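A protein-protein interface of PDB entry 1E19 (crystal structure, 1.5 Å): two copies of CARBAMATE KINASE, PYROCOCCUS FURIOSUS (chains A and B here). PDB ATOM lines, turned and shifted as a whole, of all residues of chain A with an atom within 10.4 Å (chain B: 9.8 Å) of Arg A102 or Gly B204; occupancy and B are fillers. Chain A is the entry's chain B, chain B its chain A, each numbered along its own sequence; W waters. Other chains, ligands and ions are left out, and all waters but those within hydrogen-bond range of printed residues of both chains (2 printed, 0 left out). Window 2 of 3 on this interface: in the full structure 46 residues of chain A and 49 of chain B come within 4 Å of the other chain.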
ATOM      1  N   ALA A  34       1.297   5.182  -8.846  1.00  0.00           N
ATOM      2  CA  ALA A  34       0.271   5.722  -8.011  1.00  0.00           C
ATOM      3  C   ALA A  34       0.624   5.599  -6.511  1.00  0.00           C
ATOM      4  O   ALA A  34       0.251   6.535  -5.801  1.00  0.00           O
ATOM      5  CB  ALA A  34      -1.072   5.005  -8.211  1.00  0.00           C
ATOM      6  N   ARG A  35       1.435   4.546  -6.179  1.00  0.00           N
ATOM      7  CA  ARG A  35       1.782   4.575  -4.722  1.00  0.00           C
ATOM      8  C   ARG A  35       2.731   5.697  -4.406  1.00  0.00           C
ATOM      9  O   ARG A  35       2.628   6.345  -3.318  1.00  0.00           O
ATOM     10  CB  ARG A  35       2.458   3.223  -4.426  1.00  0.00           C
ATOM     11  CG  ARG A  35       1.542   2.051  -4.395  1.00  0.00           C
ATOM     12  CD  ARG A  35       2.414   0.814  -4.110  1.00  0.00           C
ATOM     13  NE  ARG A  35       1.673  -0.373  -4.373  1.00  0.00           N
ATOM     14  CZ  ARG A  35       1.498  -1.274  -5.291  1.00  0.00           C
ATOM     15  NH1 ARG A  35       2.023  -1.307  -6.483  1.00  0.00           N
ATOM     16  NH2 ARG A  35       0.648  -2.258  -4.939  1.00  0.00           N
ATOM     17  N   ALA A  38       0.697   8.825  -4.283  1.00  0.00           N
ATOM     18  CA  ALA A  38      -0.168   8.813  -3.081  1.00  0.00           C
ATOM     19  C   ALA A  38       0.613   9.200  -1.824  1.00  0.00           C
ATOM     20  O   ALA A  38       0.158   9.940  -0.940  1.00  0.00           O
ATOM     21  CB  ALA A  38      -0.867   7.432  -2.955  1.00  0.00           C
ATOM     22  N   GLU A  39       1.887   8.806  -1.776  1.00  0.00           N
ATOM     23  CA  GLU A  39       2.696   9.218  -0.627  1.00  0.00           C
ATOM     24  C   GLU A  39       2.849  10.698  -0.524  1.00  0.00           C
ATOM     25  O   GLU A  39       2.893  11.418   0.486  1.00  0.00           O
ATOM     26  CB  GLU A  39       4.044   8.506  -0.659  1.00  0.00           C
ATOM     27  CG  GLU A  39       4.998   8.771   0.464  1.00  0.00           C
ATOM     28  CD  GLU A  39       4.516   8.098   1.799  1.00  0.00           C
ATOM     29  OE1 GLU A  39       4.014   7.021   1.696  1.00  0.00           O
ATOM     30  OE2 GLU A  39       4.742   8.952   2.673  1.00  0.00           O
ATOM     31  N   ILE A  41       0.757  13.013  -1.857  1.00  0.00           N
ATOM     32  CA  ILE A  41      -0.522  13.538  -1.444  1.00  0.00           C
ATOM     33  C   ILE A  41      -0.749  13.337   0.095  1.00  0.00           C
ATOM     34  O   ILE A  41      -1.075  14.342   0.697  1.00  0.00           O
ATOM     35  CB  ILE A  41      -1.664  12.833  -2.189  1.00  0.00           C
ATOM     36  CG1 ILE A  41      -1.619  13.247  -3.676  1.00  0.00           C
ATOM     37  CG2 ILE A  41      -3.005  13.112  -1.552  1.00  0.00           C
ATOM     38  CD1 ILE A  41      -2.143  14.639  -3.914  1.00  0.00           C
ATOM     39  N   ALA A  42      -0.330  12.225   0.604  1.00  0.00           N
ATOM     40  CA  ALA A  42      -0.469  12.060   2.113  1.00  0.00           C
ATOM     41  C   ALA A  42       0.345  13.073   2.844  1.00  0.00           C
ATOM     42  O   ALA A  42       0.115  13.505   3.993  1.00  0.00           O
ATOM     43  CB  ALA A  42       0.020  10.616   2.384  1.00  0.00           C
ATOM     44  N   GLN A  94      -6.066   7.844 -13.255  1.00  0.00           N
ATOM     45  CA  GLN A  94      -7.082   8.380 -12.309  1.00  0.00           C
ATOM     46  C   GLN A  94      -7.656   7.203 -11.558  1.00  0.00           C
ATOM     47  O   GLN A  94      -7.948   7.442 -10.352  1.00  0.00           O
ATOM     48  CB  GLN A  94      -8.136   9.269 -12.979  1.00  0.00           C
ATOM     49  CG  GLN A  94      -9.182   8.474 -13.810  1.00  0.00           C
ATOM     50  CD  GLN A  94     -10.044   9.483 -14.619  1.00  0.00           C
ATOM     51  OE1 GLN A  94      -9.516  10.377 -15.317  1.00  0.00           O
ATOM     52  NE2 GLN A  94     -11.360   9.344 -14.593  1.00  0.00           N
ATOM     53  N   GLN A  95      -7.889   6.056 -12.134  1.00  0.00           N
ATOM     54  CA  GLN A  95      -8.515   4.907 -11.366  1.00  0.00           C
ATOM     55  C   GLN A  95      -7.410   4.430 -10.394  1.00  0.00           C
ATOM     56  O   GLN A  95      -7.828   4.272  -9.197  1.00  0.00           O
ATOM     57  CB  GLN A  95      -8.848   3.846 -12.396  1.00  0.00           C
ATOM     58  CG  GLN A  95      -9.551   2.665 -11.684  1.00  0.00           C
ATOM     59  CD  GLN A  95      -9.812   1.573 -12.689  1.00  0.00           C
ATOM     60  OE1 GLN A  95      -8.953   0.724 -12.798  1.00  0.00           O
ATOM     61  NE2 GLN A  95     -10.938   1.587 -13.424  1.00  0.00           N
ATOM     62  N   ALA A  96      -6.187   4.205 -10.780  1.00  0.00           N
ATOM     63  CA  ALA A  96      -5.219   3.615  -9.770  1.00  0.00           C
ATOM     64  C   ALA A  96      -4.980   4.636  -8.671  1.00  0.00           C
ATOM     65  O   ALA A  96      -4.784   4.176  -7.495  1.00  0.00           O
ATOM     66  CB  ALA A  96      -3.926   3.381 -10.566  1.00  0.00           C
ATOM     67  N   LEU A  97      -4.831   5.913  -8.945  1.00  0.00           N
ATOM     68  CA  LEU A  97      -4.523   6.869  -7.867  1.00  0.00           C
ATOM     69  C   LEU A  97      -5.725   7.024  -7.015  1.00  0.00           C
ATOM     70  O   LEU A  97      -5.551   7.039  -5.753  1.00  0.00           O
ATOM     71  CB  LEU A  97      -4.079   8.199  -8.505  1.00  0.00           C
ATOM     72  CG  LEU A  97      -3.715   9.291  -7.471  1.00  0.00           C
ATOM     73  CD1 LEU A  97      -2.570   8.777  -6.533  1.00  0.00           C
ATOM     74  CD2 LEU A  97      -3.253  10.531  -8.250  1.00  0.00           C
ATOM     75  N   LYS A  98      -6.954   7.181  -7.411  1.00  0.00           N
ATOM     76  CA  LYS A  98      -8.125   7.272  -6.494  1.00  0.00           C
ATOM     77  C   LYS A  98      -8.200   5.971  -5.760  1.00  0.00           C
ATOM     78  O   LYS A  98      -8.486   6.129  -4.469  1.00  0.00           O
ATOM     79  CB  LYS A  98      -9.405   7.469  -7.364  1.00  0.00           C
ATOM     80  CG  LYS A  98     -10.620   7.859  -6.497  1.00  0.00           C
ATOM     81  CD  LYS A  98     -11.797   8.217  -7.330  1.00  0.00           C
ATOM     82  CE  LYS A  98     -13.055   8.496  -6.563  1.00  0.00           C
ATOM     83  NZ  LYS A  98     -12.985   9.856  -5.943  1.00  0.00           N
ATOM     84  N   ASN A  99      -7.900   4.799  -6.290  1.00  0.00           N
ATOM     85  CA  ASN A  99      -7.997   3.551  -5.476  1.00  0.00           C
ATOM     86  C   ASN A  99      -6.876   3.587  -4.443  1.00  0.00           C
ATOM     87  O   ASN A  99      -7.232   3.132  -3.279  1.00  0.00           O
ATOM     88  CB  ASN A  99      -7.826   2.389  -6.388  1.00  0.00           C
ATOM     89  CG  ASN A  99      -9.033   2.032  -7.215  1.00  0.00           C
ATOM     90  OD1 ASN A  99     -10.123   2.393  -6.847  1.00  0.00           O
ATOM     91  ND2 ASN A  99      -8.808   1.177  -8.254  1.00  0.00           N
ATOM     92  N   GLU A 100      -5.687   4.003  -4.735  1.00  0.00           N
ATOM     93  CA  GLU A 100      -4.544   3.891  -3.710  1.00  0.00           C
ATOM     94  C   GLU A 100      -4.887   4.907  -2.702  1.00  0.00           C
ATOM     95  O   GLU A 100      -4.583   4.588  -1.461  1.00  0.00           O
ATOM     96  CB  GLU A 100      -3.209   4.174  -4.421  1.00  0.00           C
ATOM     97  CG  GLU A 100      -2.081   4.418  -3.340  1.00  0.00           C
ATOM     98  CD  GLU A 100      -1.808   3.008  -2.782  1.00  0.00           C
ATOM     99  OE1 GLU A 100      -2.074   1.928  -3.355  1.00  0.00           O
ATOM    100  OE2 GLU A 100      -1.241   2.980  -1.622  1.00  0.00           O
ATOM    101  N   LEU A 101      -5.414   6.073  -2.907  1.00  0.00           N
ATOM    102  CA  LEU A 101      -5.785   7.038  -1.867  1.00  0.00           C
ATOM    103  C   LEU A 101      -6.940   6.446  -1.064  1.00  0.00           C
ATOM    104  O   LEU A 101      -6.805   6.565   0.225  1.00  0.00           O
ATOM    105  CB  LEU A 101      -6.165   8.408  -2.521  1.00  0.00           C
ATOM    106  CG  LEU A 101      -4.948   9.062  -3.216  1.00  0.00           C
ATOM    107  CD1 LEU A 101      -5.455  10.200  -4.112  1.00  0.00           C
ATOM    108  CD2 LEU A 101      -4.038   9.719  -2.091  1.00  0.00           C
ATOM    109  N   ARG A 102      -7.902   5.757  -1.619  1.00  0.00           N
ATOM    110  CA  ARG A 102      -9.007   5.219  -0.784  1.00  0.00           C
ATOM    111  C   ARG A 102      -8.330   4.142   0.073  1.00  0.00           C
ATOM    112  O   ARG A 102      -8.723   4.002   1.285  1.00  0.00           O
ATOM    113  CB  ARG A 102     -10.156   4.721  -1.662  1.00  0.00           C
ATOM    114  CG  ARG A 102     -11.293   4.135  -0.784  1.00  0.00           C
ATOM    115  CD  ARG A 102     -12.442   3.662  -1.649  1.00  0.00           C
ATOM    116  NE  ARG A 102     -13.452   4.688  -1.733  1.00  0.00           N
ATOM    117  CZ  ARG A 102     -14.650   4.472  -2.298  1.00  0.00           C
ATOM    118  NH1 ARG A 102     -14.939   3.302  -2.859  1.00  0.00           N
ATOM    119  NH2 ARG A 102     -15.513   5.474  -2.313  1.00  0.00           N
ATOM    120  N   LYS A 103      -7.413   3.339  -0.369  1.00  0.00           N
ATOM    121  CA  LYS A 103      -6.778   2.299   0.475  1.00  0.00           C
ATOM    122  C   LYS A 103      -6.073   2.947   1.638  1.00  0.00           C
ATOM    123  O   LYS A 103      -5.927   2.310   2.789  1.00  0.00           O
ATOM    124  CB  LYS A 103      -5.821   1.560  -0.453  1.00  0.00           C
ATOM    125  CG  LYS A 103      -4.987   0.508   0.232  1.00  0.00           C
ATOM    126  CD  LYS A 103      -4.375  -0.355  -0.887  1.00  0.00           C
ATOM    127  CE  LYS A 103      -3.971  -1.725  -0.373  1.00  0.00           C
ATOM    128  NZ  LYS A 103      -2.583  -2.061  -0.841  1.00  0.00           N
ATOM    129  N   ARG A 104      -5.599   4.146   1.511  1.00  0.00           N
ATOM    130  CA  ARG A 104      -4.925   4.964   2.575  1.00  0.00           C
ATOM    131  C   ARG A 104      -5.982   5.702   3.413  1.00  0.00           C
ATOM    132  O   ARG A 104      -5.530   6.577   4.172  1.00  0.00           O
ATOM    133  CB  ARG A 104      -3.862   5.860   1.974  1.00  0.00           C
ATOM    134  CG  ARG A 104      -2.767   5.015   1.360  1.00  0.00           C
ATOM    135  CD  ARG A 104      -1.591   5.825   0.910  1.00  0.00           C
ATOM    136  NE  ARG A 104      -0.628   5.071   0.116  1.00  0.00           N
ATOM    137  CZ  ARG A 104       0.700   5.307   0.224  1.00  0.00           C
ATOM    138  NH1 ARG A 104       1.205   6.173   1.116  1.00  0.00           N
ATOM    139  NH2 ARG A 104       1.466   4.562  -0.552  1.00  0.00           N
ATOM    140  N   GLY A 105      -7.233   5.461   3.278  1.00  0.00           N
ATOM    141  CA  GLY A 105      -8.315   6.122   4.027  1.00  0.00           C
ATOM    142  C   GLY A 105      -8.567   7.572   3.691  1.00  0.00           C
ATOM    143  O   GLY A 105      -9.016   8.423   4.387  1.00  0.00           O
ATOM    144  N   MET A 106      -8.107   7.974   2.442  1.00  0.00           N
ATOM    145  CA  MET A 106      -8.188   9.299   1.892  1.00  0.00           C
ATOM    146  C   MET A 106      -9.138   9.365   0.677  1.00  0.00           C
ATOM    147  O   MET A 106      -8.963   8.585  -0.302  1.00  0.00           O
ATOM    148  CB  MET A 106      -6.762   9.714   1.358  1.00  0.00           C
ATOM    149  CG  MET A 106      -5.877  10.040   2.607  1.00  0.00           C
ATOM    150  SD  MET A 106      -4.129  10.199   2.020  1.00  0.00           S
ATOM    151  CE  MET A 106      -3.924   8.572   1.362  1.00  0.00           C
ATOM    152  N   GLU A 107     -10.164  10.155   0.769  1.00  0.00           N
ATOM    153  CA  GLU A 107     -11.107  10.263  -0.408  1.00  0.00           C
ATOM    154  C   GLU A 107     -10.680  11.501  -1.179  1.00  0.00           C
ATOM    155  O   GLU A 107     -10.608  12.559  -0.583  1.00  0.00           O
ATOM    156  CB  GLU A 107     -12.510  10.423   0.165  1.00  0.00           C
ATOM    157  CG  GLU A 107     -13.074   9.148   0.789  1.00  0.00           C
ATOM    158  CD  GLU A 107     -13.382   7.995  -0.138  1.00  0.00           C
ATOM    159  OE1 GLU A 107     -13.925   8.169  -1.250  1.00  0.00           O
ATOM    160  OE2 GLU A 107     -13.085   6.837   0.273  1.00  0.00           O
ATOM    161  N   LYS A 108     -10.298  11.346  -2.496  1.00  0.00           N
ATOM    162  CA  LYS A 108      -9.939  12.574  -3.187  1.00  0.00           C
ATOM    163  C   LYS A 108     -10.587  12.433  -4.592  1.00  0.00           C
ATOM    164  O   LYS A 108     -10.741  11.298  -5.011  1.00  0.00           O
ATOM    165  CB  LYS A 108      -8.423  12.793  -3.491  1.00  0.00           C
ATOM    166  CG  LYS A 108      -7.586  12.881  -2.222  1.00  0.00           C
ATOM    167  CD  LYS A 108      -7.623  14.232  -1.563  1.00  0.00           C
ATOM    168  CE  LYS A 108      -7.060  14.050  -0.133  1.00  0.00           C
ATOM    169  NZ  LYS A 108      -6.920  15.393   0.506  1.00  0.00           N
ATOM    170  N   LYS A 109     -10.763  13.596  -5.183  1.00  0.00           N
ATOM    171  CA  LYS A 109     -11.313  13.546  -6.611  1.00  0.00           C
ATOM    172  C   LYS A 109     -10.088  13.621  -7.543  1.00  0.00           C
ATOM    173  O   LYS A 109      -9.096  14.366  -7.301  1.00  0.00           O
ATOM    174  CB  LYS A 109     -12.103  14.842  -6.797  1.00  0.00           C
ATOM    175  CG  LYS A 109     -13.421  14.764  -5.952  1.00  0.00           C
ATOM    176  CD  LYS A 109     -14.134  16.119  -5.938  1.00  0.00           C
ATOM    177  CE  LYS A 109     -13.514  17.003  -4.860  1.00  0.00           C
ATOM    178  NZ  LYS A 109     -14.182  16.757  -3.529  1.00  0.00           N
ATOM    179  N   VAL A 110     -10.105  12.734  -8.543  1.00  0.00           N
ATOM    180  CA  VAL A 110      -8.960  12.576  -9.452  1.00  0.00           C
ATOM    181  C   VAL A 110      -9.565  12.495 -10.869  1.00  0.00           C
ATOM    182  O   VAL A 110     -10.314  11.534 -11.161  1.00  0.00           O
ATOM    183  CB  VAL A 110      -8.139  11.332  -9.158  1.00  0.00           C
ATOM    184  CG1 VAL A 110      -6.889  11.360 -10.017  1.00  0.00           C
ATOM    185  CG2 VAL A 110      -7.782  11.211  -7.661  1.00  0.00           C
ATOM    186  N   ILE A 188      -7.263  16.562  -7.932  1.00  0.00           N
ATOM    187  CA  ILE A 188      -6.034  16.087  -8.562  1.00  0.00           C
ATOM    188  C   ILE A 188      -6.318  15.895 -10.093  1.00  0.00           C
ATOM    189  O   ILE A 188      -7.167  15.112 -10.457  1.00  0.00           O
ATOM    190  CB  ILE A 188      -5.466  14.781  -7.986  1.00  0.00           C
ATOM    191  CG1 ILE A 188      -5.243  14.979  -6.420  1.00  0.00           C
ATOM    192  CG2 ILE A 188      -4.211  14.313  -8.711  1.00  0.00           C
ATOM    193  CD1 ILE A 188      -5.338  13.598  -5.721  1.00  0.00           C
ATOM    194  N   ILE B 118     -20.392   3.574 -12.905  1.00  0.00           N
ATOM    195  CA  ILE B 118     -20.551   2.419 -11.960  1.00  0.00           C
ATOM    196  C   ILE B 118     -21.833   1.649 -12.295  1.00  0.00           C
ATOM    197  O   ILE B 118     -22.921   2.099 -12.615  1.00  0.00           O
ATOM    198  CB  ILE B 118     -20.759   3.071 -10.544  1.00  0.00           C
ATOM    199  CG1 ILE B 118     -19.502   3.892 -10.176  1.00  0.00           C
ATOM    200  CG2 ILE B 118     -20.961   1.942  -9.512  1.00  0.00           C
ATOM    201  CD1 ILE B 118     -19.863   4.908  -9.051  1.00  0.00           C
ATOM    202  N   LYS B 121     -22.093  -5.130  -9.622  1.00  0.00           N
ATOM    203  CA  LYS B 121     -21.454  -6.419 -10.040  1.00  0.00           C
ATOM    204  C   LYS B 121     -22.417  -7.605  -9.921  1.00  0.00           C
ATOM    205  O   LYS B 121     -22.147  -8.580 -10.630  1.00  0.00           O
ATOM    206  CB  LYS B 121     -20.247  -6.601  -9.193  1.00  0.00           C
ATOM    207  CG  LYS B 121     -20.587  -6.710  -7.743  1.00  0.00           C
ATOM    208  CD  LYS B 121     -19.163  -6.661  -7.087  1.00  0.00           C
ATOM    209  CE  LYS B 121     -19.384  -6.601  -5.592  1.00  0.00           C
ATOM    210  NZ  LYS B 121     -19.552  -5.140  -5.236  1.00  0.00           N
ATOM    211  N   VAL B 174     -18.388   7.846 -11.348  1.00  0.00           N
ATOM    212  CA  VAL B 174     -17.372   8.090 -10.342  1.00  0.00           C
ATOM    213  C   VAL B 174     -17.163   9.609 -10.204  1.00  0.00           C
ATOM    214  O   VAL B 174     -16.918  10.126  -9.076  1.00  0.00           O
ATOM    215  CB  VAL B 174     -16.065   7.328 -10.674  1.00  0.00           C
ATOM    216  CG1 VAL B 174     -14.927   7.739  -9.744  1.00  0.00           C
ATOM    217  CG2 VAL B 174     -16.311   5.768 -10.597  1.00  0.00           C
ATOM    218  N   GLU B 177     -19.456  14.291  -8.833  1.00  0.00           N
ATOM    219  CA  GLU B 177     -19.351  15.549  -8.061  1.00  0.00           C
ATOM    220  C   GLU B 177     -18.522  16.548  -8.767  1.00  0.00           C
ATOM    221  O   GLU B 177     -18.876  17.772  -8.741  1.00  0.00           O
ATOM    222  CB  GLU B 177     -18.885  15.096  -6.690  1.00  0.00           C
ATOM    223  CG  GLU B 177     -20.006  14.539  -5.822  1.00  0.00           C
ATOM    224  CD  GLU B 177     -19.494  14.186  -4.433  1.00  0.00           C
ATOM    225  OE1 GLU B 177     -18.302  14.316  -4.075  1.00  0.00           O
ATOM    226  OE2 GLU B 177     -20.367  13.766  -3.629  1.00  0.00           O
ATOM    227  N   VAL B 199     -17.401   0.262 -14.868  1.00  0.00           N
ATOM    228  CA  VAL B 199     -16.618  -0.147 -13.680  1.00  0.00           C
ATOM    229  C   VAL B 199     -17.556  -0.683 -12.601  1.00  0.00           C
ATOM    230  O   VAL B 199     -18.732  -0.333 -12.534  1.00  0.00           O
ATOM    231  CB  VAL B 199     -15.800   1.013 -13.070  1.00  0.00           C
ATOM    232  CG1 VAL B 199     -14.810   1.582 -14.118  1.00  0.00           C
ATOM    233  CG2 VAL B 199     -16.653   2.131 -12.479  1.00  0.00           C
ATOM    234  N   ILE B 200     -16.907  -1.573 -11.829  1.00  0.00           N
ATOM    235  CA  ILE B 200     -17.647  -2.057 -10.593  1.00  0.00           C
ATOM    236  C   ILE B 200     -16.795  -1.568  -9.431  1.00  0.00           C
ATOM    237  O   ILE B 200     -15.632  -1.211  -9.486  1.00  0.00           O
ATOM    238  CB  ILE B 200     -17.737  -3.612 -10.513  1.00  0.00           C
ATOM    239  CG1 ILE B 200     -16.352  -4.239 -10.716  1.00  0.00           C
ATOM    240  CG2 ILE B 200     -18.665  -4.062 -11.675  1.00  0.00           C
ATOM    241  CD1 ILE B 200     -16.291  -5.770 -10.490  1.00  0.00           C
ATOM    242  N   LEU B 201     -17.500  -1.680  -8.240  1.00  0.00           N
ATOM    243  CA  LEU B 201     -16.812  -1.372  -6.972  1.00  0.00           C
ATOM    244  C   LEU B 201     -16.595  -2.642  -6.110  1.00  0.00           C
ATOM    245  O   LEU B 201     -17.666  -3.302  -5.909  1.00  0.00           O
ATOM    246  CB  LEU B 201     -17.678  -0.393  -6.170  1.00  0.00           C
ATOM    247  CG  LEU B 201     -18.111   0.825  -6.947  1.00  0.00           C
ATOM    248  CD1 LEU B 201     -18.997   1.744  -6.092  1.00  0.00           C
ATOM    249  CD2 LEU B 201     -16.979   1.659  -7.547  1.00  0.00           C
ATOM    250  N   GLU B 202     -15.406  -2.999  -5.805  1.00  0.00           N
ATOM    251  CA  GLU B 202     -15.212  -4.291  -5.050  1.00  0.00           C
ATOM    252  C   GLU B 202     -14.212  -4.015  -3.928  1.00  0.00           C
ATOM    253  O   GLU B 202     -13.033  -3.658  -4.100  1.00  0.00           O
ATOM    254  CB  GLU B 202     -14.556  -5.283  -6.002  1.00  0.00           C
ATOM    255  CG  GLU B 202     -14.410  -6.678  -5.295  1.00  0.00           C
ATOM    256  CD  GLU B 202     -14.338  -7.703  -6.428  1.00  0.00           C
ATOM    257  OE1 GLU B 202     -13.312  -7.690  -7.149  1.00  0.00           O
ATOM    258  OE2 GLU B 202     -15.300  -8.488  -6.629  1.00  0.00           O
ATOM    259  N   ASP B 203     -14.764  -4.081  -2.671  1.00  0.00           N
ATOM    260  CA  ASP B 203     -13.874  -3.876  -1.529  1.00  0.00           C
ATOM    261  C   ASP B 203     -13.229  -2.463  -1.608  1.00  0.00           C
ATOM    262  O   ASP B 203     -12.056  -2.286  -1.260  1.00  0.00           O
ATOM    263  CB  ASP B 203     -12.785  -4.941  -1.449  1.00  0.00           C
ATOM    264  CG  ASP B 203     -13.331  -6.337  -1.154  1.00  0.00           C
ATOM    265  OD1 ASP B 203     -14.254  -6.447  -0.306  1.00  0.00           O
ATOM    266  OD2 ASP B 203     -12.879  -7.345  -1.751  1.00  0.00           O
ATOM    267  N   GLY B 204     -14.111  -1.585  -2.043  1.00  0.00           N
ATOM    268  CA  GLY B 204     -13.768  -0.174  -2.185  1.00  0.00           C
ATOM    269  C   GLY B 204     -12.945   0.155  -3.430  1.00  0.00           C
ATOM    270  O   GLY B 204     -12.813   1.366  -3.699  1.00  0.00           O
ATOM    271  N   GLU B 205     -12.499  -0.809  -4.182  1.00  0.00           N
ATOM    272  CA  GLU B 205     -11.670  -0.556  -5.379  1.00  0.00           C
ATOM    273  C   GLU B 205     -12.530  -0.541  -6.635  1.00  0.00           C
ATOM    274  O   GLU B 205     -13.450  -1.337  -6.805  1.00  0.00           O
ATOM    275  CB  GLU B 205     -10.826  -1.861  -5.492  1.00  0.00           C
ATOM    276  CG  GLU B 205      -9.771  -1.762  -6.528  1.00  0.00           C
ATOM    277  CD  GLU B 205      -8.766  -2.884  -6.744  1.00  0.00           C
ATOM    278  OE1 GLU B 205      -8.765  -3.663  -5.728  1.00  0.00           O
ATOM    279  OE2 GLU B 205      -8.055  -2.946  -7.785  1.00  0.00           O
ATOM    280  N   ILE B 206     -12.219   0.543  -7.406  1.00  0.00           N
ATOM    281  CA  ILE B 206     -12.895   0.680  -8.756  1.00  0.00           C
ATOM    282  C   ILE B 206     -12.097  -0.203  -9.750  1.00  0.00           C
ATOM    283  O   ILE B 206     -10.890  -0.096  -9.878  1.00  0.00           O
ATOM    284  CB  ILE B 206     -12.757   2.141  -9.153  1.00  0.00           C
ATOM    285  CG1 ILE B 206     -13.467   3.080  -8.192  1.00  0.00           C
ATOM    286  CG2 ILE B 206     -13.471   2.336 -10.548  1.00  0.00           C
ATOM    287  CD1 ILE B 206     -12.858   4.483  -8.380  1.00  0.00           C
ATOM    288  N   LYS B 207     -12.918  -1.075 -10.391  1.00  0.00           N
ATOM    289  CA  LYS B 207     -12.264  -2.016 -11.357  1.00  0.00           C
ATOM    290  C   LYS B 207     -13.018  -1.949 -12.700  1.00  0.00           C
ATOM    291  O   LYS B 207     -14.251  -2.052 -12.718  1.00  0.00           O
ATOM    292  CB  LYS B 207     -12.370  -3.492 -10.841  1.00  0.00           C
ATOM    293  CG  LYS B 207     -11.601  -3.656  -9.524  1.00  0.00           C
ATOM    294  CD  LYS B 207     -11.720  -5.136  -8.990  1.00  0.00           C
ATOM    295  CE  LYS B 207     -10.965  -5.100  -7.637  1.00  0.00           C
ATOM    296  NZ  LYS B 207     -10.643  -6.530  -7.212  1.00  0.00           N
HETATM  297  O   HOH W   1     -11.738   3.552  -4.935  1.00  0.00           O
HETATM  298  O   HOH W   2      -8.604  -1.664 -10.150  1.00  0.00           O
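O of Gly B204 lies within hydrogen-bond range of NH1 of Arg A102 (3.0 Å). The backbone NH (N) of Ile B206 lies within hydrogen-bond range of the side-chain amide oxygen (OD1) of Asn A99, 2.9 Å away.
The side-chain carboxylate of Glu B205 lies within salt-bridge range of the side-chain amino group of Lys B207 (3.7 Å). O of Gln A95 lies close to ND2 of Asn A99, 3.4 Å away. The backbone carbonyl oxygen of Lys A108 sits at hydrogen-bond distance from the side-chain amino group of Lys A98 (2.8 Å). OE2 of Glu A107 lies within salt-bridge range of NE of Arg A102, at 3.0 Å.
Among the printed residues, pairs that only touch across the chains: Gln A95 with Val B199 (3.9 Å), Gln A95 with Ile B206 (3.4 Å), Lys A98 with Val B174 (3.8 Å) and Asn A99 with Glu B205 (3.5 Å).
Of chain B, only Gly B204 (3.0 Å) comes within 4 Å of Arg A102. Of chain A, only Arg A102 (3.0 Å) comes within 4 Å of Gly B204. Leu A101 touches none of the printed residues of chain B. Gly A105 touches none of the printed residues of chain B. No residue of chain A comes within 4 Å of Asp B203. Of the printed residues of chain B, Asn A99 touches Glu B205 (3.5 Å) and Ile B206 (2.9 Å). Of the printed residues of chain B, Gln A95 touches Val B199 and Ile B206. Printed residues of chain A within 4 Å of Glu B205: Asn A99. The nearest residue of chain B that does not touch Arg A102 is Glu B205 (5.0 Å). The nearest residue of chain A that does not touch Gly B204 is Asn A99 (4.3 Å).
Of the 13 printed residues of chain B, 5 touch a printed residue of chain A. Along chain A the printed residues that touch a printed residue of chain B span positions 95 to 102. Among the printed residues, no Asp or Glu carboxylate lies within 4 Å of a Lys or Arg side-chain nitrogen of the other chain.
No position is printed for both chains. Of the 6 pairs that touch across the chains among the printed residues, none has its exchanged pair printed and touching as well.
Water W1 lies within hydrogen-bond range of O of Gly B204 (2.7 Å) and OD1 of Asn A99 (2.8 Å). Water W2 lies within hydrogen-bond range of the side-chain carboxylate of Glu B205 (2.7 Å), the backbone carbonyl oxygen of Ile B206 (2.8 Å) and the side-chain amide nitrogen of Asn A99 (3.4 Å).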
